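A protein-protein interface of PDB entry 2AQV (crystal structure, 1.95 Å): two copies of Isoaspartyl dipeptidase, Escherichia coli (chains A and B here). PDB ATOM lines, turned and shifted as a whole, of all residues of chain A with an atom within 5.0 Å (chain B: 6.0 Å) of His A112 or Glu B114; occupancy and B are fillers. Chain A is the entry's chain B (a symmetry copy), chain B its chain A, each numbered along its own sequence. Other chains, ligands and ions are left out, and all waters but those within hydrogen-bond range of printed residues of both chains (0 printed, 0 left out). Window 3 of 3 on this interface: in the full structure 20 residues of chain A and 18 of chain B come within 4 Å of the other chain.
The backbone carbonyl oxygen (O) of Ile A109 lies within hydrogen-bond range of a ring nitrogen (NE2) of His A112 (3.1 Å).
The side-chain hydroxyl (OG) of Ser B115 is in hydrogen-bond range of the backbone carbonyl oxygen (O) of Ser A110 (2.6 Å).
Of the 12 printed residues of chain B, 4 touch a printed residue of chain A.
Printed residues of chain B that touch a printed residue of chain A: His B112, Glu B114, Ser B115 and Ala B118.
Hydrophobic or aromatic side chains of chain B within 4 Å of the printed part of chain A: His B112 and Ala B118.
Of the 10 printed residues of chain A, 4 touch a printed residue of chain B.
Hydrophobic or aromatic side chains of chain A that line the printed part of chain B: His A112.
Among the printed residues, no Asp or Glu carboxylate lies within 4 Å of a Lys or Arg side-chain nitrogen of the other chain.
Of the printed residues of chain B, Ile A109 touches Glu B114 (3.4 Å).
Printed residues of chain B within 4 Å of Ser A110: Ser B115 (2.6 Å) and Ala B118 (3.98 Å).
Of the printed residues of chain B, His A112 touches His B112, Glu B114 and Ser B115.
Printed residues of chain B within 4 Å of Ser A115: His B112 (3.7 Å).
Printed residues of chain A within 4 Å of His B112: His A112 (3.4 Å) and Ser A115 (3.7 Å).
Of the printed residues of chain A, Ala B118 touches Ser A110 (3.98 Å).
Lys B119 touches none of the printed residues of chain A.
The nearest printed residue of chain B that does not touch Ser A110 is Glu B114 (4.1 Å).
His B112 touches its own counterpart, His A112.
His A112 touches Glu B114, but with the chains exchanged Glu A114 does not touch His B112 (4.1 Å).
His A112 touches Ser B115, and with the chains exchanged Ser A115 touches His B112.
5 positions are printed for both chains.
Ile A109 touches Glu B114.
Ala B118 touches Ser A110.
His A112 touches His B112.
Glu B114 touches His A112.
CE1 of His A112 touches OG of Ser B115 (3.4 Å).
His B112 touches Ser A115.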
ATOM      1  N   ILE A  72      11.447 -26.065  -2.956  1.00  0.00           N
ATOM      2  CA  ILE A  72      12.029 -25.804  -4.259  1.00  0.00           C
ATOM      3  C   ILE A  72      13.046 -26.870  -4.683  1.00  0.00           C
ATOM      4  O   ILE A  72      13.613 -26.784  -5.766  1.00  0.00           O
ATOM      5  CB  ILE A  72      12.593 -24.391  -4.474  1.00  0.00           C
ATOM      6  CG1 ILE A  72      13.750 -24.098  -3.520  1.00  0.00           C
ATOM      7  CG2 ILE A  72      11.490 -23.323  -4.458  1.00  0.00           C
ATOM      8  CD1 ILE A  72      14.509 -22.815  -3.890  1.00  0.00           C
ATOM      9  N   LEU A 104      15.402 -23.927   3.226  1.00  0.00           N
ATOM     10  CA  LEU A 104      16.628 -24.248   2.483  1.00  0.00           C
ATOM     11  C   LEU A 104      17.551 -25.046   3.420  1.00  0.00           C
ATOM     12  O   LEU A 104      17.381 -24.994   4.658  1.00  0.00           O
ATOM     13  CB  LEU A 104      17.337 -22.936   2.011  1.00  0.00           C
ATOM     14  CG  LEU A 104      16.501 -22.093   1.024  1.00  0.00           C
ATOM     15  CD1 LEU A 104      17.333 -20.952   0.434  1.00  0.00           C
ATOM     16  CD2 LEU A 104      15.937 -22.943  -0.121  1.00  0.00           C
ATOM     17  N   ILE A 109      23.593 -21.147  -2.426  1.00  0.00           N
ATOM     18  CA  ILE A 109      24.367 -20.563  -3.529  1.00  0.00           C
ATOM     19  C   ILE A 109      23.503 -20.712  -4.792  1.00  0.00           C
ATOM     20  O   ILE A 109      23.216 -19.760  -5.535  1.00  0.00           O
ATOM     21  CB  ILE A 109      25.724 -21.244  -3.766  1.00  0.00           C
ATOM     22  CG1 ILE A 109      26.709 -21.137  -2.594  1.00  0.00           C
ATOM     23  CG2 ILE A 109      26.373 -20.727  -5.055  1.00  0.00           C
ATOM     24  CD1 ILE A 109      27.189 -19.722  -2.380  1.00  0.00           C
ATOM     25  N   SER A 110      23.014 -21.947  -5.018  1.00  0.00           N
ATOM     26  CA  SER A 110      22.179 -22.147  -6.200  1.00  0.00           C
ATOM     27  C   SER A 110      20.708 -22.086  -5.835  1.00  0.00           C
ATOM     28  O   SER A 110      19.856 -22.171  -6.711  1.00  0.00           O
ATOM     29  CB  SER A 110      22.496 -23.469  -6.886  1.00  0.00           C
ATOM     30  OG  SER A 110      21.812 -24.513  -6.146  1.00  0.00           O
ATOM     31  N   ARG A 111      20.430 -21.961  -4.521  1.00  0.00           N
ATOM     32  CA  ARG A 111      19.086 -21.890  -3.972  1.00  0.00           C
ATOM     33  C   ARG A 111      18.948 -20.538  -3.299  1.00  0.00           C
ATOM     34  O   ARG A 111      19.879 -20.144  -2.581  1.00  0.00           O
ATOM     35  CB  ARG A 111      18.833 -22.981  -2.921  1.00  0.00           C
ATOM     36  CG  ARG A 111      19.059 -24.392  -3.462  1.00  0.00           C
ATOM     37  CD  ARG A 111      18.194 -24.804  -4.670  1.00  0.00           C
ATOM     38  NE  ARG A 111      18.296 -26.265  -4.883  1.00  0.00           N
ATOM     39  CZ  ARG A 111      17.599 -26.969  -5.740  1.00  0.00           C
ATOM     40  NH1 ARG A 111      16.742 -26.374  -6.546  1.00  0.00           N
ATOM     41  NH2 ARG A 111      17.774 -28.308  -5.779  1.00  0.00           N
ATOM     42  N   HIS A 112      17.801 -19.865  -3.531  1.00  0.00           N
ATOM     43  CA  HIS A 112      17.519 -18.517  -3.043  1.00  0.00           C
ATOM     44  C   HIS A 112      16.139 -18.324  -2.365  1.00  0.00           C
ATOM     45  O   HIS A 112      15.158 -18.886  -2.819  1.00  0.00           O
ATOM     46  CB  HIS A 112      17.626 -17.533  -4.254  1.00  0.00           C
ATOM     47  CG  HIS A 112      18.907 -17.697  -5.003  1.00  0.00           C
ATOM     48  ND1 HIS A 112      19.081 -18.721  -5.940  1.00  0.00           N
ATOM     49  CD2 HIS A 112      20.076 -17.008  -4.935  1.00  0.00           C
ATOM     50  CE1 HIS A 112      20.306 -18.634  -6.429  1.00  0.00           C
ATOM     51  NE2 HIS A 112      20.935 -17.631  -5.820  1.00  0.00           N
ATOM     52  N   PRO A 113      16.081 -17.513  -1.285  1.00  0.00           N
ATOM     53  CA  PRO A 113      14.827 -17.277  -0.572  1.00  0.00           C
ATOM     54  C   PRO A 113      13.774 -16.736  -1.513  1.00  0.00           C
ATOM     55  O   PRO A 113      12.607 -17.070  -1.347  1.00  0.00           O
ATOM     56  CB  PRO A 113      15.114 -16.302   0.584  1.00  0.00           C
ATOM     57  CG  PRO A 113      16.617 -16.070   0.615  1.00  0.00           C
ATOM     58  CD  PRO A 113      17.210 -16.823  -0.589  1.00  0.00           C
ATOM     59  N   GLU A 114      14.196 -15.936  -2.513  1.00  0.00           N
ATOM     60  CA  GLU A 114      13.245 -15.390  -3.457  1.00  0.00           C
ATOM     61  C   GLU A 114      12.568 -16.468  -4.240  1.00  0.00           C
ATOM     62  O   GLU A 114      11.402 -16.334  -4.553  1.00  0.00           O
ATOM     63  CB  GLU A 114      13.818 -14.369  -4.457  1.00  0.00           C
ATOM     64  CG  GLU A 114      14.282 -13.113  -3.729  1.00  0.00           C
ATOM     65  CD  GLU A 114      15.705 -13.239  -3.246  1.00  0.00           C
ATOM     66  OE1 GLU A 114      16.325 -14.291  -3.156  1.00  0.00           O
ATOM     67  OE2 GLU A 114      16.157 -12.070  -2.883  1.00  0.00           O
ATOM     68  N   SER A 115      13.315 -17.523  -4.584  1.00  0.00           N
ATOM     69  CA  SER A 115      12.679 -18.616  -5.321  1.00  0.00           C
ATOM     70  C   SER A 115      11.710 -19.372  -4.398  1.00  0.00           C
ATOM     71  O   SER A 115      10.603 -19.789  -4.786  1.00  0.00           O
ATOM     72  CB  SER A 115      13.713 -19.610  -5.825  1.00  0.00           C
ATOM     73  OG  SER A 115      14.698 -18.923  -6.596  1.00  0.00           O
ATOM     74  N   LEU A 116      12.156 -19.562  -3.158  1.00  0.00           N
ATOM     75  CA  LEU A 116      11.406 -20.270  -2.165  1.00  0.00           C
ATOM     76  C   LEU A 116      10.090 -19.527  -1.890  1.00  0.00           C
ATOM     77  O   LEU A 116       9.007 -20.111  -1.782  1.00  0.00           O
ATOM     78  CB  LEU A 116      12.242 -20.568  -0.888  1.00  0.00           C
ATOM     79  CG  LEU A 116      11.425 -21.223   0.241  1.00  0.00           C
ATOM     80  CD1 LEU A 116      10.917 -22.618  -0.193  1.00  0.00           C
ATOM     81  CD2 LEU A 116      12.354 -21.359   1.433  1.00  0.00           C
ATOM     82  N   HIS B 112      17.786 -17.256 -10.968  1.00  0.00           N
ATOM     83  CA  HIS B 112      19.119 -16.674 -10.826  1.00  0.00           C
ATOM     84  C   HIS B 112      20.151 -17.386 -11.689  1.00  0.00           C
ATOM     85  O   HIS B 112      20.075 -18.609 -11.883  1.00  0.00           O
ATOM     86  CB  HIS B 112      19.545 -16.789  -9.349  1.00  0.00           C
ATOM     87  CG  HIS B 112      18.471 -16.253  -8.434  1.00  0.00           C
ATOM     88  ND1 HIS B 112      18.579 -15.030  -7.750  1.00  0.00           N
ATOM     89  CD2 HIS B 112      17.270 -16.789  -8.096  1.00  0.00           C
ATOM     90  CE1 HIS B 112      17.457 -14.864  -7.026  1.00  0.00           C
ATOM     91  NE2 HIS B 112      16.668 -15.910  -7.213  1.00  0.00           N
ATOM     92  N   PRO B 113      21.155 -16.612 -12.151  1.00  0.00           N
ATOM     93  CA  PRO B 113      22.225 -17.168 -12.980  1.00  0.00           C
ATOM     94  C   PRO B 113      22.986 -18.224 -12.220  1.00  0.00           C
ATOM     95  O   PRO B 113      23.447 -19.145 -12.836  1.00  0.00           O
ATOM     96  CB  PRO B 113      23.176 -16.025 -13.386  1.00  0.00           C
ATOM     97  CG  PRO B 113      22.636 -14.756 -12.747  1.00  0.00           C
ATOM     98  CD  PRO B 113      21.341 -15.121 -12.004  1.00  0.00           C
ATOM     99  N   GLU B 114      23.132 -18.086 -10.897  1.00  0.00           N
ATOM    100  CA  GLU B 114      23.847 -19.134 -10.161  1.00  0.00           C
ATOM    101  C   GLU B 114      23.126 -20.469 -10.260  1.00  0.00           C
ATOM    102  O   GLU B 114      23.774 -21.523 -10.286  1.00  0.00           O
ATOM    103  CB  GLU B 114      24.056 -18.768  -8.674  1.00  0.00           C
ATOM    104  CG  GLU B 114      24.940 -17.532  -8.598  1.00  0.00           C
ATOM    105  CD  GLU B 114      24.136 -16.266  -8.707  1.00  0.00           C
ATOM    106  OE1 GLU B 114      22.937 -16.247  -8.923  1.00  0.00           O
ATOM    107  OE2 GLU B 114      24.884 -15.197  -8.569  1.00  0.00           O
ATOM    108  N   SER B 115      21.803 -20.422 -10.271  1.00  0.00           N
ATOM    109  CA  SER B 115      21.029 -21.665 -10.372  1.00  0.00           C
ATOM    110  C   SER B 115      21.218 -22.261 -11.753  1.00  0.00           C
ATOM    111  O   SER B 115      21.509 -23.435 -11.927  1.00  0.00           O
ATOM    112  CB  SER B 115      19.572 -21.342 -10.164  1.00  0.00           C
ATOM    113  OG  SER B 115      19.398 -20.795  -8.874  1.00  0.00           O
ATOM    114  N   LEU B 116      21.078 -21.404 -12.761  1.00  0.00           N
ATOM    115  CA  LEU B 116      21.271 -21.756 -14.128  1.00  0.00           C
ATOM    116  C   LEU B 116      22.662 -22.380 -14.293  1.00  0.00           C
ATOM    117  O   LEU B 116      22.846 -23.401 -14.942  1.00  0.00           O
ATOM    118  CB  LEU B 116      21.079 -20.487 -15.029  1.00  0.00           C
ATOM    119  CG  LEU B 116      21.234 -20.793 -16.554  1.00  0.00           C
ATOM    120  CD1 LEU B 116      20.316 -21.949 -17.027  1.00  0.00           C
ATOM    121  CD2 LEU B 116      20.892 -19.555 -17.385  1.00  0.00           C
ATOM    122  N   LEU B 117      23.688 -21.742 -13.706  1.00  0.00           N
ATOM    123  CA  LEU B 117      25.027 -22.293 -13.845  1.00  0.00           C
ATOM    124  C   LEU B 117      25.142 -23.701 -13.271  1.00  0.00           C
ATOM    125  O   LEU B 117      25.773 -24.608 -13.863  1.00  0.00           O
ATOM    126  CB  LEU B 117      26.086 -21.317 -13.266  1.00  0.00           C
ATOM    127  CG  LEU B 117      27.515 -21.885 -13.200  1.00  0.00           C
ATOM    128  CD1 LEU B 117      28.129 -21.947 -14.601  1.00  0.00           C
ATOM    129  CD2 LEU B 117      28.369 -20.965 -12.309  1.00  0.00           C
ATOM    130  N   ALA B 118      24.540 -23.908 -12.111  1.00  0.00           N
ATOM    131  CA  ALA B 118      24.590 -25.246 -11.507  1.00  0.00           C
ATOM    132  C   ALA B 118      23.946 -26.303 -12.391  1.00  0.00           C
ATOM    133  O   ALA B 118      24.478 -27.398 -12.577  1.00  0.00           O
ATOM    134  CB  ALA B 118      23.916 -25.297 -10.129  1.00  0.00           C
ATOM    135  N   LYS B 119      22.771 -25.973 -12.908  1.00  0.00           N
ATOM    136  CA  LYS B 119      22.010 -26.900 -13.779  1.00  0.00           C
ATOM    137  C   LYS B 119      22.803 -27.245 -15.043  1.00  0.00           C
ATOM    138  O   LYS B 119      22.839 -28.404 -15.532  1.00  0.00           O
ATOM    139  CB  LYS B 119      20.670 -26.274 -14.151  1.00  0.00           C
ATOM    140  CG  LYS B 119      19.850 -27.177 -15.082  1.00  0.00           C
ATOM    141  CD  LYS B 119      19.487 -28.561 -14.516  1.00  0.00           C
ATOM    142  CE  LYS B 119      18.502 -29.235 -15.451  1.00  0.00           C
ATOM    143  NZ  LYS B 119      17.837 -30.362 -14.815  1.00  0.00           N
ATOM    144  N   MET B 132      25.787 -21.419 -21.077  1.00  0.00           N
ATOM    145  CA  MET B 132      24.694 -20.547 -20.717  1.00  0.00           C
ATOM    146  C   MET B 132      25.062 -19.120 -21.082  1.00  0.00           C
ATOM    147  O   MET B 132      26.222 -18.826 -21.368  1.00  0.00           O
ATOM    148  CB  MET B 132      24.417 -20.631 -19.188  1.00  0.00           C
ATOM    149  CG  MET B 132      25.620 -20.208 -18.330  1.00  0.00           C
ATOM    150  SD  MET B 132      25.247 -20.043 -16.539  1.00  0.00           S
ATOM    151  CE  MET B 132      24.367 -18.439 -16.436  1.00  0.00           C
ATOM    152  N   THR B 143      23.827 -10.198 -13.062  1.00  0.00           N
ATOM    153  CA  THR B 143      24.884 -11.140 -13.373  1.00  0.00           C
ATOM    154  C   THR B 143      25.352 -11.852 -12.136  1.00  0.00           C
ATOM    155  O   THR B 143      24.920 -11.575 -11.027  1.00  0.00           O
ATOM    156  CB  THR B 143      26.103 -10.377 -13.943  1.00  0.00           C
ATOM    157  OG1 THR B 143      26.528  -9.483 -12.941  1.00  0.00           O
ATOM    158  CG2 THR B 143      25.819  -9.577 -15.197  1.00  0.00           C
ATOM    159  N   ILE B 144      26.291 -12.752 -12.347  1.00  0.00           N
ATOM    160  CA  ILE B 144      26.896 -13.503 -11.265  1.00  0.00           C
ATOM    161  C   ILE B 144      28.008 -12.730 -10.564  1.00  0.00           C
ATOM    162  O   ILE B 144      28.057 -12.658  -9.326  1.00  0.00           O
ATOM    163  CB  ILE B 144      27.482 -14.815 -11.772  1.00  0.00           C
ATOM    164  CG1 ILE B 144      26.389 -15.735 -12.292  1.00  0.00           C
ATOM    165  CG2 ILE B 144      28.275 -15.507 -10.667  1.00  0.00           C
ATOM    166  CD1 ILE B 144      26.974 -16.790 -13.228  1.00  0.00           C
ATOM    167  N   THR B 145      28.919 -12.134 -11.344  1.00  0.00           N
ATOM    168  CA  THR B 145      30.016 -11.457 -10.684  1.00  0.00           C
ATOM    169  C   THR B 145      29.809  -9.973 -10.516  1.00  0.00           C
ATOM    170  O   THR B 145      30.695  -9.289  -9.981  1.00  0.00           O
ATOM    171  CB  THR B 145      31.331 -11.658 -11.445  1.00  0.00           C
ATOM    172  OG1 THR B 145      31.190 -10.944 -12.689  1.00  0.00           O
ATOM    173  CG2 THR B 145      31.629 -13.133 -11.660  1.00  0.00           C
